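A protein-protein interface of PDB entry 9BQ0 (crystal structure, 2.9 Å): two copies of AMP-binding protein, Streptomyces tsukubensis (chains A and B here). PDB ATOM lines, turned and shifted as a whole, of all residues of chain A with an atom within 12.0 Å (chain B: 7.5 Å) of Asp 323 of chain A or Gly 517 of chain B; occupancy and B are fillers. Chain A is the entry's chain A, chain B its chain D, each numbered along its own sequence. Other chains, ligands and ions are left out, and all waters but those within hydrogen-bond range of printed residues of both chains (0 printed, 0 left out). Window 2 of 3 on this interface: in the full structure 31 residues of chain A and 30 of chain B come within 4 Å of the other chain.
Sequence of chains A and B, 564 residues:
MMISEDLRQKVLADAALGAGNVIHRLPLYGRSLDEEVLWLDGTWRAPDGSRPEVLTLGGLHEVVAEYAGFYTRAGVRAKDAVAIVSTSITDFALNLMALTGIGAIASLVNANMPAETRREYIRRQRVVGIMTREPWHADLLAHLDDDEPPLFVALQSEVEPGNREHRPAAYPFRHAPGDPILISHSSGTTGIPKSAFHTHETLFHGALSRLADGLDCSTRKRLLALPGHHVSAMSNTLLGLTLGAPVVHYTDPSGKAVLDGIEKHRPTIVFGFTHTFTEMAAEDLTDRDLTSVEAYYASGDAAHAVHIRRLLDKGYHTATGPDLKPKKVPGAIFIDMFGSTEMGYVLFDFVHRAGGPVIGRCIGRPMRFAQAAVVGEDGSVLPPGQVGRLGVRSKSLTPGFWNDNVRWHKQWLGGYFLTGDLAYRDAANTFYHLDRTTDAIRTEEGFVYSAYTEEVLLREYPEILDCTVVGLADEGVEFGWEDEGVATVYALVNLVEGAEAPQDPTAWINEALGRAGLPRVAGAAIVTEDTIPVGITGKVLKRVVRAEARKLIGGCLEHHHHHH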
ATOM      1  N   HIS A 317       7.671  18.851  18.464  1.00  0.00           N
ATOM      2  CA  HIS A 317       7.142  18.944  17.117  1.00  0.00           C
ATOM      3  C   HIS A 317       8.289  19.403  16.236  1.00  0.00           C
ATOM      4  O   HIS A 317       9.098  20.229  16.647  1.00  0.00           O
ATOM      5  CB  HIS A 317       5.925  19.877  17.053  1.00  0.00           C
ATOM      6  CG  HIS A 317       6.242  21.330  17.142  1.00  0.00           C
ATOM      7  ND1 HIS A 317       6.774  22.044  16.089  1.00  0.00           N
ATOM      8  CD2 HIS A 317       6.063  22.216  18.150  1.00  0.00           C
ATOM      9  CE1 HIS A 317       6.929  23.305  16.452  1.00  0.00           C
ATOM     10  NE2 HIS A 317       6.505  23.435  17.698  1.00  0.00           N
ATOM     11  N   THR A 318       8.388  18.806  15.050  1.00  0.00           N
ATOM     12  CA  THR A 318       9.476  19.114  14.136  1.00  0.00           C
ATOM     13  C   THR A 318       9.116  20.404  13.417  1.00  0.00           C
ATOM     14  O   THR A 318       7.974  20.582  12.977  1.00  0.00           O
ATOM     15  CB  THR A 318       9.693  17.963  13.131  1.00  0.00           C
ATOM     16  OG1 THR A 318       9.706  16.680  13.803  1.00  0.00           O
ATOM     17  CG2 THR A 318      10.997  18.160  12.308  1.00  0.00           C
ATOM     18  N   ALA A 319      10.083  21.312  13.317  1.00  0.00           N
ATOM     19  CA  ALA A 319       9.875  22.577  12.638  1.00  0.00           C
ATOM     20  C   ALA A 319      11.060  22.805  11.722  1.00  0.00           C
ATOM     21  O   ALA A 319      12.009  22.013  11.702  1.00  0.00           O
ATOM     22  CB  ALA A 319       9.727  23.738  13.614  1.00  0.00           C
ATOM     23  N   THR A 320      10.942  23.850  10.896  1.00  0.00           N
ATOM     24  CA  THR A 320      11.981  24.247   9.923  1.00  0.00           C
ATOM     25  C   THR A 320      12.619  25.522  10.446  1.00  0.00           C
ATOM     26  O   THR A 320      11.919  26.543  10.476  1.00  0.00           O
ATOM     27  CB  THR A 320      11.374  24.466   8.539  1.00  0.00           C
ATOM     28  OG1 THR A 320      11.072  23.178   8.005  1.00  0.00           O
ATOM     29  CG2 THR A 320      12.294  25.222   7.607  1.00  0.00           C
ATOM     30  N   GLY A 321      13.880  25.462  10.850  1.00  0.00           N
ATOM     31  CA  GLY A 321      14.554  26.615  11.461  1.00  0.00           C
ATOM     32  C   GLY A 321      15.084  27.581  10.433  1.00  0.00           C
ATOM     33  O   GLY A 321      14.742  27.436   9.252  1.00  0.00           O
ATOM     34  N   PRO A 322      15.885  28.577  10.847  1.00  0.00           N
ATOM     35  CA  PRO A 322      16.518  29.515   9.910  1.00  0.00           C
ATOM     36  C   PRO A 322      17.725  28.916   9.191  1.00  0.00           C
ATOM     37  O   PRO A 322      18.231  29.524   8.241  1.00  0.00           O
ATOM     38  CB  PRO A 322      16.895  30.708  10.797  1.00  0.00           C
ATOM     39  CG  PRO A 322      16.556  30.294  12.244  1.00  0.00           C
ATOM     40  CD  PRO A 322      16.319  28.820  12.231  1.00  0.00           C
ATOM     41  N   ASP A 323      18.229  27.766   9.628  1.00  0.00           N
ATOM     42  CA  ASP A 323      19.214  27.069   8.817  1.00  0.00           C
ATOM     43  C   ASP A 323      18.568  26.412   7.610  1.00  0.00           C
ATOM     44  O   ASP A 323      19.278  25.898   6.722  1.00  0.00           O
ATOM     45  CB  ASP A 323      19.922  26.056   9.706  1.00  0.00           C
ATOM     46  CG  ASP A 323      18.951  25.093  10.387  1.00  0.00           C
ATOM     47  OD1 ASP A 323      17.952  25.565  11.003  1.00  0.00           O
ATOM     48  OD2 ASP A 323      19.249  23.874  10.372  1.00  0.00           O
ATOM     49  N   LEU A 324      17.234  26.488   7.556  1.00  0.00           N
ATOM     50  CA  LEU A 324      16.390  25.880   6.536  1.00  0.00           C
ATOM     51  C   LEU A 324      16.432  24.369   6.602  1.00  0.00           C
ATOM     52  O   LEU A 324      16.194  23.695   5.591  1.00  0.00           O
ATOM     53  CB  LEU A 324      16.783  26.342   5.132  1.00  0.00           C
ATOM     54  CG  LEU A 324      16.488  27.802   4.781  1.00  0.00           C
ATOM     55  CD1 LEU A 324      16.259  28.000   3.276  1.00  0.00           C
ATOM     56  CD2 LEU A 324      15.273  28.303   5.571  1.00  0.00           C
ATOM     57  N   LYS A 325      16.664  23.849   7.802  1.00  0.00           N
ATOM     58  CA  LYS A 325      16.753  22.425   8.067  1.00  0.00           C
ATOM     59  C   LYS A 325      15.841  22.095   9.229  1.00  0.00           C
ATOM     60  O   LYS A 325      15.535  22.971  10.044  1.00  0.00           O
ATOM     61  CB  LYS A 325      18.192  22.010   8.408  1.00  0.00           C
ATOM     62  CG  LYS A 325      19.256  22.695   7.568  1.00  0.00           C
ATOM     63  CD  LYS A 325      20.431  21.731   7.287  1.00  0.00           C
ATOM     64  CE  LYS A 325      21.809  22.419   7.476  1.00  0.00           C
ATOM     65  NZ  LYS A 325      22.957  21.514   7.181  1.00  0.00           N
ATOM     66  N   PRO A 326      15.408  20.827   9.368  1.00  0.00           N
ATOM     67  CA  PRO A 326      14.484  20.460  10.429  1.00  0.00           C
ATOM     68  C   PRO A 326      15.016  20.891  11.801  1.00  0.00           C
ATOM     69  O   PRO A 326      16.211  21.009  11.941  1.00  0.00           O
ATOM     70  CB  PRO A 326      14.407  18.937  10.331  1.00  0.00           C
ATOM     71  CG  PRO A 326      14.766  18.641   8.900  1.00  0.00           C
ATOM     72  CD  PRO A 326      15.802  19.684   8.550  1.00  0.00           C
ATOM     73  N   LYS A 327      14.137  21.105  12.777  1.00  0.00           N
ATOM     74  CA  LYS A 327      14.535  21.569  14.124  1.00  0.00           C
ATOM     75  C   LYS A 327      13.538  21.081  15.168  1.00  0.00           C
ATOM     76  O   LYS A 327      12.418  21.567  15.161  1.00  0.00           O
ATOM     77  CB  LYS A 327      14.586  23.094  14.180  1.00  0.00           C
ATOM     78  CG  LYS A 327      14.826  23.665  15.569  1.00  0.00           C
ATOM     79  CD  LYS A 327      15.896  22.920  16.332  1.00  0.00           C
ATOM     80  CE  LYS A 327      16.465  23.718  17.484  1.00  0.00           C
ATOM     81  NZ  LYS A 327      17.622  24.533  17.052  1.00  0.00           N
ATOM     82  N   LYS A 328      13.958  20.203  16.071  1.00  0.00           N
ATOM     83  CA  LYS A 328      13.089  19.746  17.177  1.00  0.00           C
ATOM     84  C   LYS A 328      12.731  20.958  18.027  1.00  0.00           C
ATOM     85  O   LYS A 328      13.647  21.697  18.397  1.00  0.00           O
ATOM     86  CB  LYS A 328      13.753  18.653  18.012  1.00  0.00           C
ATOM     87  CG  LYS A 328      12.780  17.698  18.680  1.00  0.00           C
ATOM     88  CD  LYS A 328      12.321  16.606  17.754  1.00  0.00           C
ATOM     89  CE  LYS A 328      10.860  16.269  17.935  1.00  0.00           C
ATOM     90  NZ  LYS A 328       9.998  17.333  17.375  1.00  0.00           N
ATOM     91  N   VAL A 329      11.458  21.148  18.309  1.00  0.00           N
ATOM     92  CA  VAL A 329      10.901  22.254  19.088  1.00  0.00           C
ATOM     93  C   VAL A 329      10.116  21.715  20.279  1.00  0.00           C
ATOM     94  O   VAL A 329       9.492  20.658  20.154  1.00  0.00           O
ATOM     95  CB  VAL A 329      10.015  23.116  18.173  1.00  0.00           C
ATOM     96  CG1 VAL A 329       9.202  24.155  18.935  1.00  0.00           C
ATOM     97  CG2 VAL A 329      10.840  23.781  17.108  1.00  0.00           C
ATOM     98  N   PHE B 447      23.920  25.020  -0.292  1.00  0.00           N
ATOM     99  CA  PHE B 447      23.177  25.861  -1.266  1.00  0.00           C
ATOM    100  C   PHE B 447      22.810  27.188  -0.608  1.00  0.00           C
ATOM    101  O   PHE B 447      22.679  27.189   0.623  1.00  0.00           O
ATOM    102  CB  PHE B 447      21.930  25.145  -1.789  1.00  0.00           C
ATOM    103  CG  PHE B 447      22.264  23.906  -2.572  1.00  0.00           C
ATOM    104  CD1 PHE B 447      22.610  23.989  -3.909  1.00  0.00           C
ATOM    105  CD2 PHE B 447      22.168  22.655  -1.988  1.00  0.00           C
ATOM    106  CE1 PHE B 447      22.883  22.845  -4.640  1.00  0.00           C
ATOM    107  CE2 PHE B 447      22.439  21.513  -2.723  1.00  0.00           C
ATOM    108  CZ  PHE B 447      22.796  21.612  -4.045  1.00  0.00           C
ATOM    109  N   TYR B 449      20.015  30.325  -0.927  1.00  0.00           N
ATOM    110  CA  TYR B 449      18.823  31.008  -1.482  1.00  0.00           C
ATOM    111  C   TYR B 449      19.036  32.481  -1.160  1.00  0.00           C
ATOM    112  O   TYR B 449      19.029  32.770   0.019  1.00  0.00           O
ATOM    113  CB  TYR B 449      17.604  30.301  -0.899  1.00  0.00           C
ATOM    114  CG  TYR B 449      17.743  28.805  -0.982  1.00  0.00           C
ATOM    115  CD1 TYR B 449      18.299  28.209  -2.100  1.00  0.00           C
ATOM    116  CD2 TYR B 449      17.388  27.993   0.076  1.00  0.00           C
ATOM    117  CE1 TYR B 449      18.464  26.840  -2.182  1.00  0.00           C
ATOM    118  CE2 TYR B 449      17.545  26.619   0.013  1.00  0.00           C
ATOM    119  CZ  TYR B 449      18.084  26.041  -1.121  1.00  0.00           C
ATOM    120  OH  TYR B 449      18.240  24.688  -1.190  1.00  0.00           O
ATOM    121  N   TYR B 452      16.040  34.990   0.489  1.00  0.00           N
ATOM    122  CA  TYR B 452      15.979  34.718   1.913  1.00  0.00           C
ATOM    123  C   TYR B 452      17.235  35.242   2.596  1.00  0.00           C
ATOM    124  O   TYR B 452      17.156  36.086   3.489  1.00  0.00           O
ATOM    125  CB  TYR B 452      15.807  33.211   2.106  1.00  0.00           C
ATOM    126  CG  TYR B 452      16.062  32.681   3.494  1.00  0.00           C
ATOM    127  CD1 TYR B 452      15.290  33.089   4.569  1.00  0.00           C
ATOM    128  CD2 TYR B 452      17.053  31.747   3.711  1.00  0.00           C
ATOM    129  CE1 TYR B 452      15.506  32.597   5.808  1.00  0.00           C
ATOM    130  CE2 TYR B 452      17.278  31.248   4.937  1.00  0.00           C
ATOM    131  CZ  TYR B 452      16.508  31.676   5.997  1.00  0.00           C
ATOM    132  OH  TYR B 452      16.727  31.190   7.276  1.00  0.00           O
ATOM    133  N   GLU B 511      28.344  37.837  10.870  1.00  0.00           N
ATOM    134  CA  GLU B 511      27.888  37.617  12.230  1.00  0.00           C
ATOM    135  C   GLU B 511      26.387  37.474  12.254  1.00  0.00           C
ATOM    136  O   GLU B 511      25.861  36.661  13.019  1.00  0.00           O
ATOM    137  CB  GLU B 511      28.349  38.785  13.139  1.00  0.00           C
ATOM    138  CG  GLU B 511      28.442  38.445  14.667  1.00  0.00           C
ATOM    139  CD  GLU B 511      29.066  39.552  15.551  1.00  0.00           C
ATOM    140  OE1 GLU B 511      29.631  40.512  14.982  1.00  0.00           O
ATOM    141  OE2 GLU B 511      28.981  39.442  16.811  1.00  0.00           O
ATOM    142  N   ALA B 512      25.693  38.229  11.399  1.00  0.00           N
ATOM    143  CA  ALA B 512      24.262  38.020  11.220  1.00  0.00           C
ATOM    144  C   ALA B 512      23.979  36.592  10.786  1.00  0.00           C
ATOM    145  O   ALA B 512      23.154  35.902  11.393  1.00  0.00           O
ATOM    146  CB  ALA B 512      23.699  39.010  10.195  1.00  0.00           C
ATOM    147  N   LEU B 513      24.672  36.125   9.743  1.00  0.00           N
ATOM    148  CA  LEU B 513      24.445  34.766   9.263  1.00  0.00           C
ATOM    149  C   LEU B 513      24.737  33.737  10.365  1.00  0.00           C
ATOM    150  O   LEU B 513      23.912  32.855  10.637  1.00  0.00           O
ATOM    151  CB  LEU B 513      25.250  34.502   7.973  1.00  0.00           C
ATOM    152  CG  LEU B 513      25.087  35.534   6.828  1.00  0.00           C
ATOM    153  CD1 LEU B 513      26.064  35.324   5.697  1.00  0.00           C
ATOM    154  CD2 LEU B 513      23.684  35.599   6.268  1.00  0.00           C
ATOM    155  N   GLY B 514      25.884  33.857  11.043  1.00  0.00           N
ATOM    156  CA  GLY B 514      26.200  32.900  12.095  1.00  0.00           C
ATOM    157  C   GLY B 514      25.152  32.859  13.189  1.00  0.00           C
ATOM    158  O   GLY B 514      24.635  31.800  13.531  1.00  0.00           O
ATOM    159  N   ARG B 515      24.780  34.015  13.715  1.00  0.00           N
ATOM    160  CA  ARG B 515      23.749  34.033  14.743  1.00  0.00           C
ATOM    161  C   ARG B 515      22.497  33.347  14.242  1.00  0.00           C
ATOM    162  O   ARG B 515      21.927  32.490  14.928  1.00  0.00           O
ATOM    163  CB  ARG B 515      23.449  35.477  15.136  1.00  0.00           C
ATOM    164  CG  ARG B 515      22.767  35.674  16.475  1.00  0.00           C
ATOM    165  CD  ARG B 515      22.183  37.080  16.534  1.00  0.00           C
ATOM    166  NE  ARG B 515      20.998  37.158  15.703  1.00  0.00           N
ATOM    167  CZ  ARG B 515      19.865  36.555  16.008  1.00  0.00           C
ATOM    168  NH1 ARG B 515      19.732  35.891  17.143  1.00  0.00           N
ATOM    169  NH2 ARG B 515      18.853  36.600  15.146  1.00  0.00           N
ATOM    170  N   ALA B 516      22.095  33.676  13.008  1.00  0.00           N
ATOM    171  CA  ALA B 516      20.857  33.197  12.415  1.00  0.00           C
ATOM    172  C   ALA B 516      20.974  31.763  11.936  1.00  0.00           C
ATOM    173  O   ALA B 516      19.952  31.084  11.776  1.00  0.00           O
ATOM    174  CB  ALA B 516      20.460  34.098  11.252  1.00  0.00           C
ATOM    175  N   GLY B 517      22.180  31.309  11.632  1.00  0.00           N
ATOM    176  CA  GLY B 517      22.418  29.910  11.392  1.00  0.00           C
ATOM    177  C   GLY B 517      22.715  29.529   9.995  1.00  0.00           C
ATOM    178  O   GLY B 517      22.551  28.355   9.663  1.00  0.00           O
ATOM    179  N   LEU B 518      23.133  30.467   9.152  1.00  0.00           N
ATOM    180  CA  LEU B 518      23.251  30.318   7.710  1.00  0.00           C
ATOM    181  C   LEU B 518      24.705  30.178   7.263  1.00  0.00           C
ATOM    182  O   LEU B 518      25.626  30.556   7.987  1.00  0.00           O
ATOM    183  CB  LEU B 518      22.596  31.534   7.038  1.00  0.00           C
ATOM    184  CG  LEU B 518      21.088  31.585   7.373  1.00  0.00           C
ATOM    185  CD1 LEU B 518      20.625  32.629   8.407  1.00  0.00           C
ATOM    186  CD2 LEU B 518      20.280  31.782   6.108  1.00  0.00           C
ATOM    187  N   PRO B 519      24.949  29.619   6.080  1.00  0.00           N
ATOM    188  CA  PRO B 519      26.291  29.697   5.502  1.00  0.00           C
ATOM    189  C   PRO B 519      26.677  31.156   5.302  1.00  0.00           C
ATOM    190  O   PRO B 519      25.830  32.044   5.160  1.00  0.00           O
ATOM    191  CB  PRO B 519      26.149  28.971   4.158  1.00  0.00           C
ATOM    192  CG  PRO B 519      24.710  29.201   3.781  1.00  0.00           C
ATOM    193  CD  PRO B 519      23.964  29.123   5.097  1.00  0.00           C
ATOM    194  N   ARG B 520      27.972  31.403   5.268  1.00  0.00           N
ATOM    195  CA  ARG B 520      28.456  32.759   5.336  1.00  0.00           C
ATOM    196  C   ARG B 520      29.210  33.125   4.080  1.00  0.00           C
ATOM    197  O   ARG B 520      29.773  32.270   3.391  1.00  0.00           O
ATOM    198  CB  ARG B 520      29.338  32.935   6.556  1.00  0.00           C
ATOM    199  CG  ARG B 520      28.914  32.083   7.758  1.00  0.00           C
ATOM    200  CD  ARG B 520      29.635  32.584   9.010  1.00  0.00           C
ATOM    201  NE  ARG B 520      29.087  32.040  10.242  1.00  0.00           N
ATOM    202  CZ  ARG B 520      29.248  30.786  10.633  1.00  0.00           C
ATOM    203  NH1 ARG B 520      29.887  29.905   9.878  1.00  0.00           N
ATOM    204  NH2 ARG B 520      28.748  30.407  11.808  1.00  0.00           N
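The backbone carbonyl oxygen (O) of Pro 322 of chain A sits at hydrogen-bond distance from the side-chain hydroxyl (OH) of Tyr 452 of chain B, at 2.4 Å.
Of the 13 printed residues of chain B, 5 touch a printed residue of chain A.
Printed residues of chain A that touch a printed residue of chain B: Pro 322, Asp 323 and Leu 324.
Hydrophobic or aromatic side chains of chain A that line the printed part of chain B: Pro 322 and Leu 324.
Among the printed residues, 6 pairs touch across the chains.
Among the printed residues, no Asp or Glu carboxylate lies within 4 Å of a Lys or Arg side-chain nitrogen of the other chain.
The backbone NH of Leu 518 of chain B sits at hydrogen-bond distance from the backbone carbonyl oxygen of Leu 513 of chain B, at 2.9 Å.
Asp 323 of chain A touches just one residue of chain B: Gly 517 (3.5 Å).
Of chain A, only Asp 323 comes within 4 Å of Gly 517 of chain B.
Arg 515 of chain B touches none of the printed residues of chain A.
Of the printed residues of chain A, Leu 518 of chain B touches Pro 322 (3.6 Å).
Pro 519 of chain B touches none of the printed residues of chain A.
Of the printed residues of chain B, Leu 324 of chain A touches Tyr 449 (3.4 Å) and Tyr 452 (3.5 Å).
Printed residues of chain A within 4 Å of Tyr 452 of chain B: Pro 322 and Leu 324.
Of the printed residues of chain B, Pro 322 of chain A touches Tyr 452 (2.4 Å), Ala 516 (3.2 Å) and Leu 518 (3.6 Å).
Of the printed residues of chain A, Tyr 449 of chain B touches Leu 324.
Ala 512 of chain B touches none of the printed residues of chain A.
Gly 321 of chain A touches none of the printed residues of chain B.
The nearest residue of chain B that does not touch Asp 323 of chain A is Ala 516 of chain B (4.3 Å).
The nearest residue of chain A that does not touch Gly 517 of chain B is Pro 322 of chain A (4.7 Å).
The nearest printed residue of chain A that does not touch Tyr 449 of chain B is Asp 323 of chain A (7.0 Å).
Among the printed residues, pairs that only touch across the chains: Pro 322 of chain A with Ala 516 of chain B, Leu 324 of chain A with Tyr 449 of chain B, Asp 323 of chain A with Gly 517 of chain B, Leu 324 of chain A with Tyr 452 of chain B and Pro 322 of chain A with Leu 518 of chain B.
No position is printed for both chains.
Of the 6 pairs that touch across the chains among the printed residues, none has its exchanged pair printed and touching as well.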
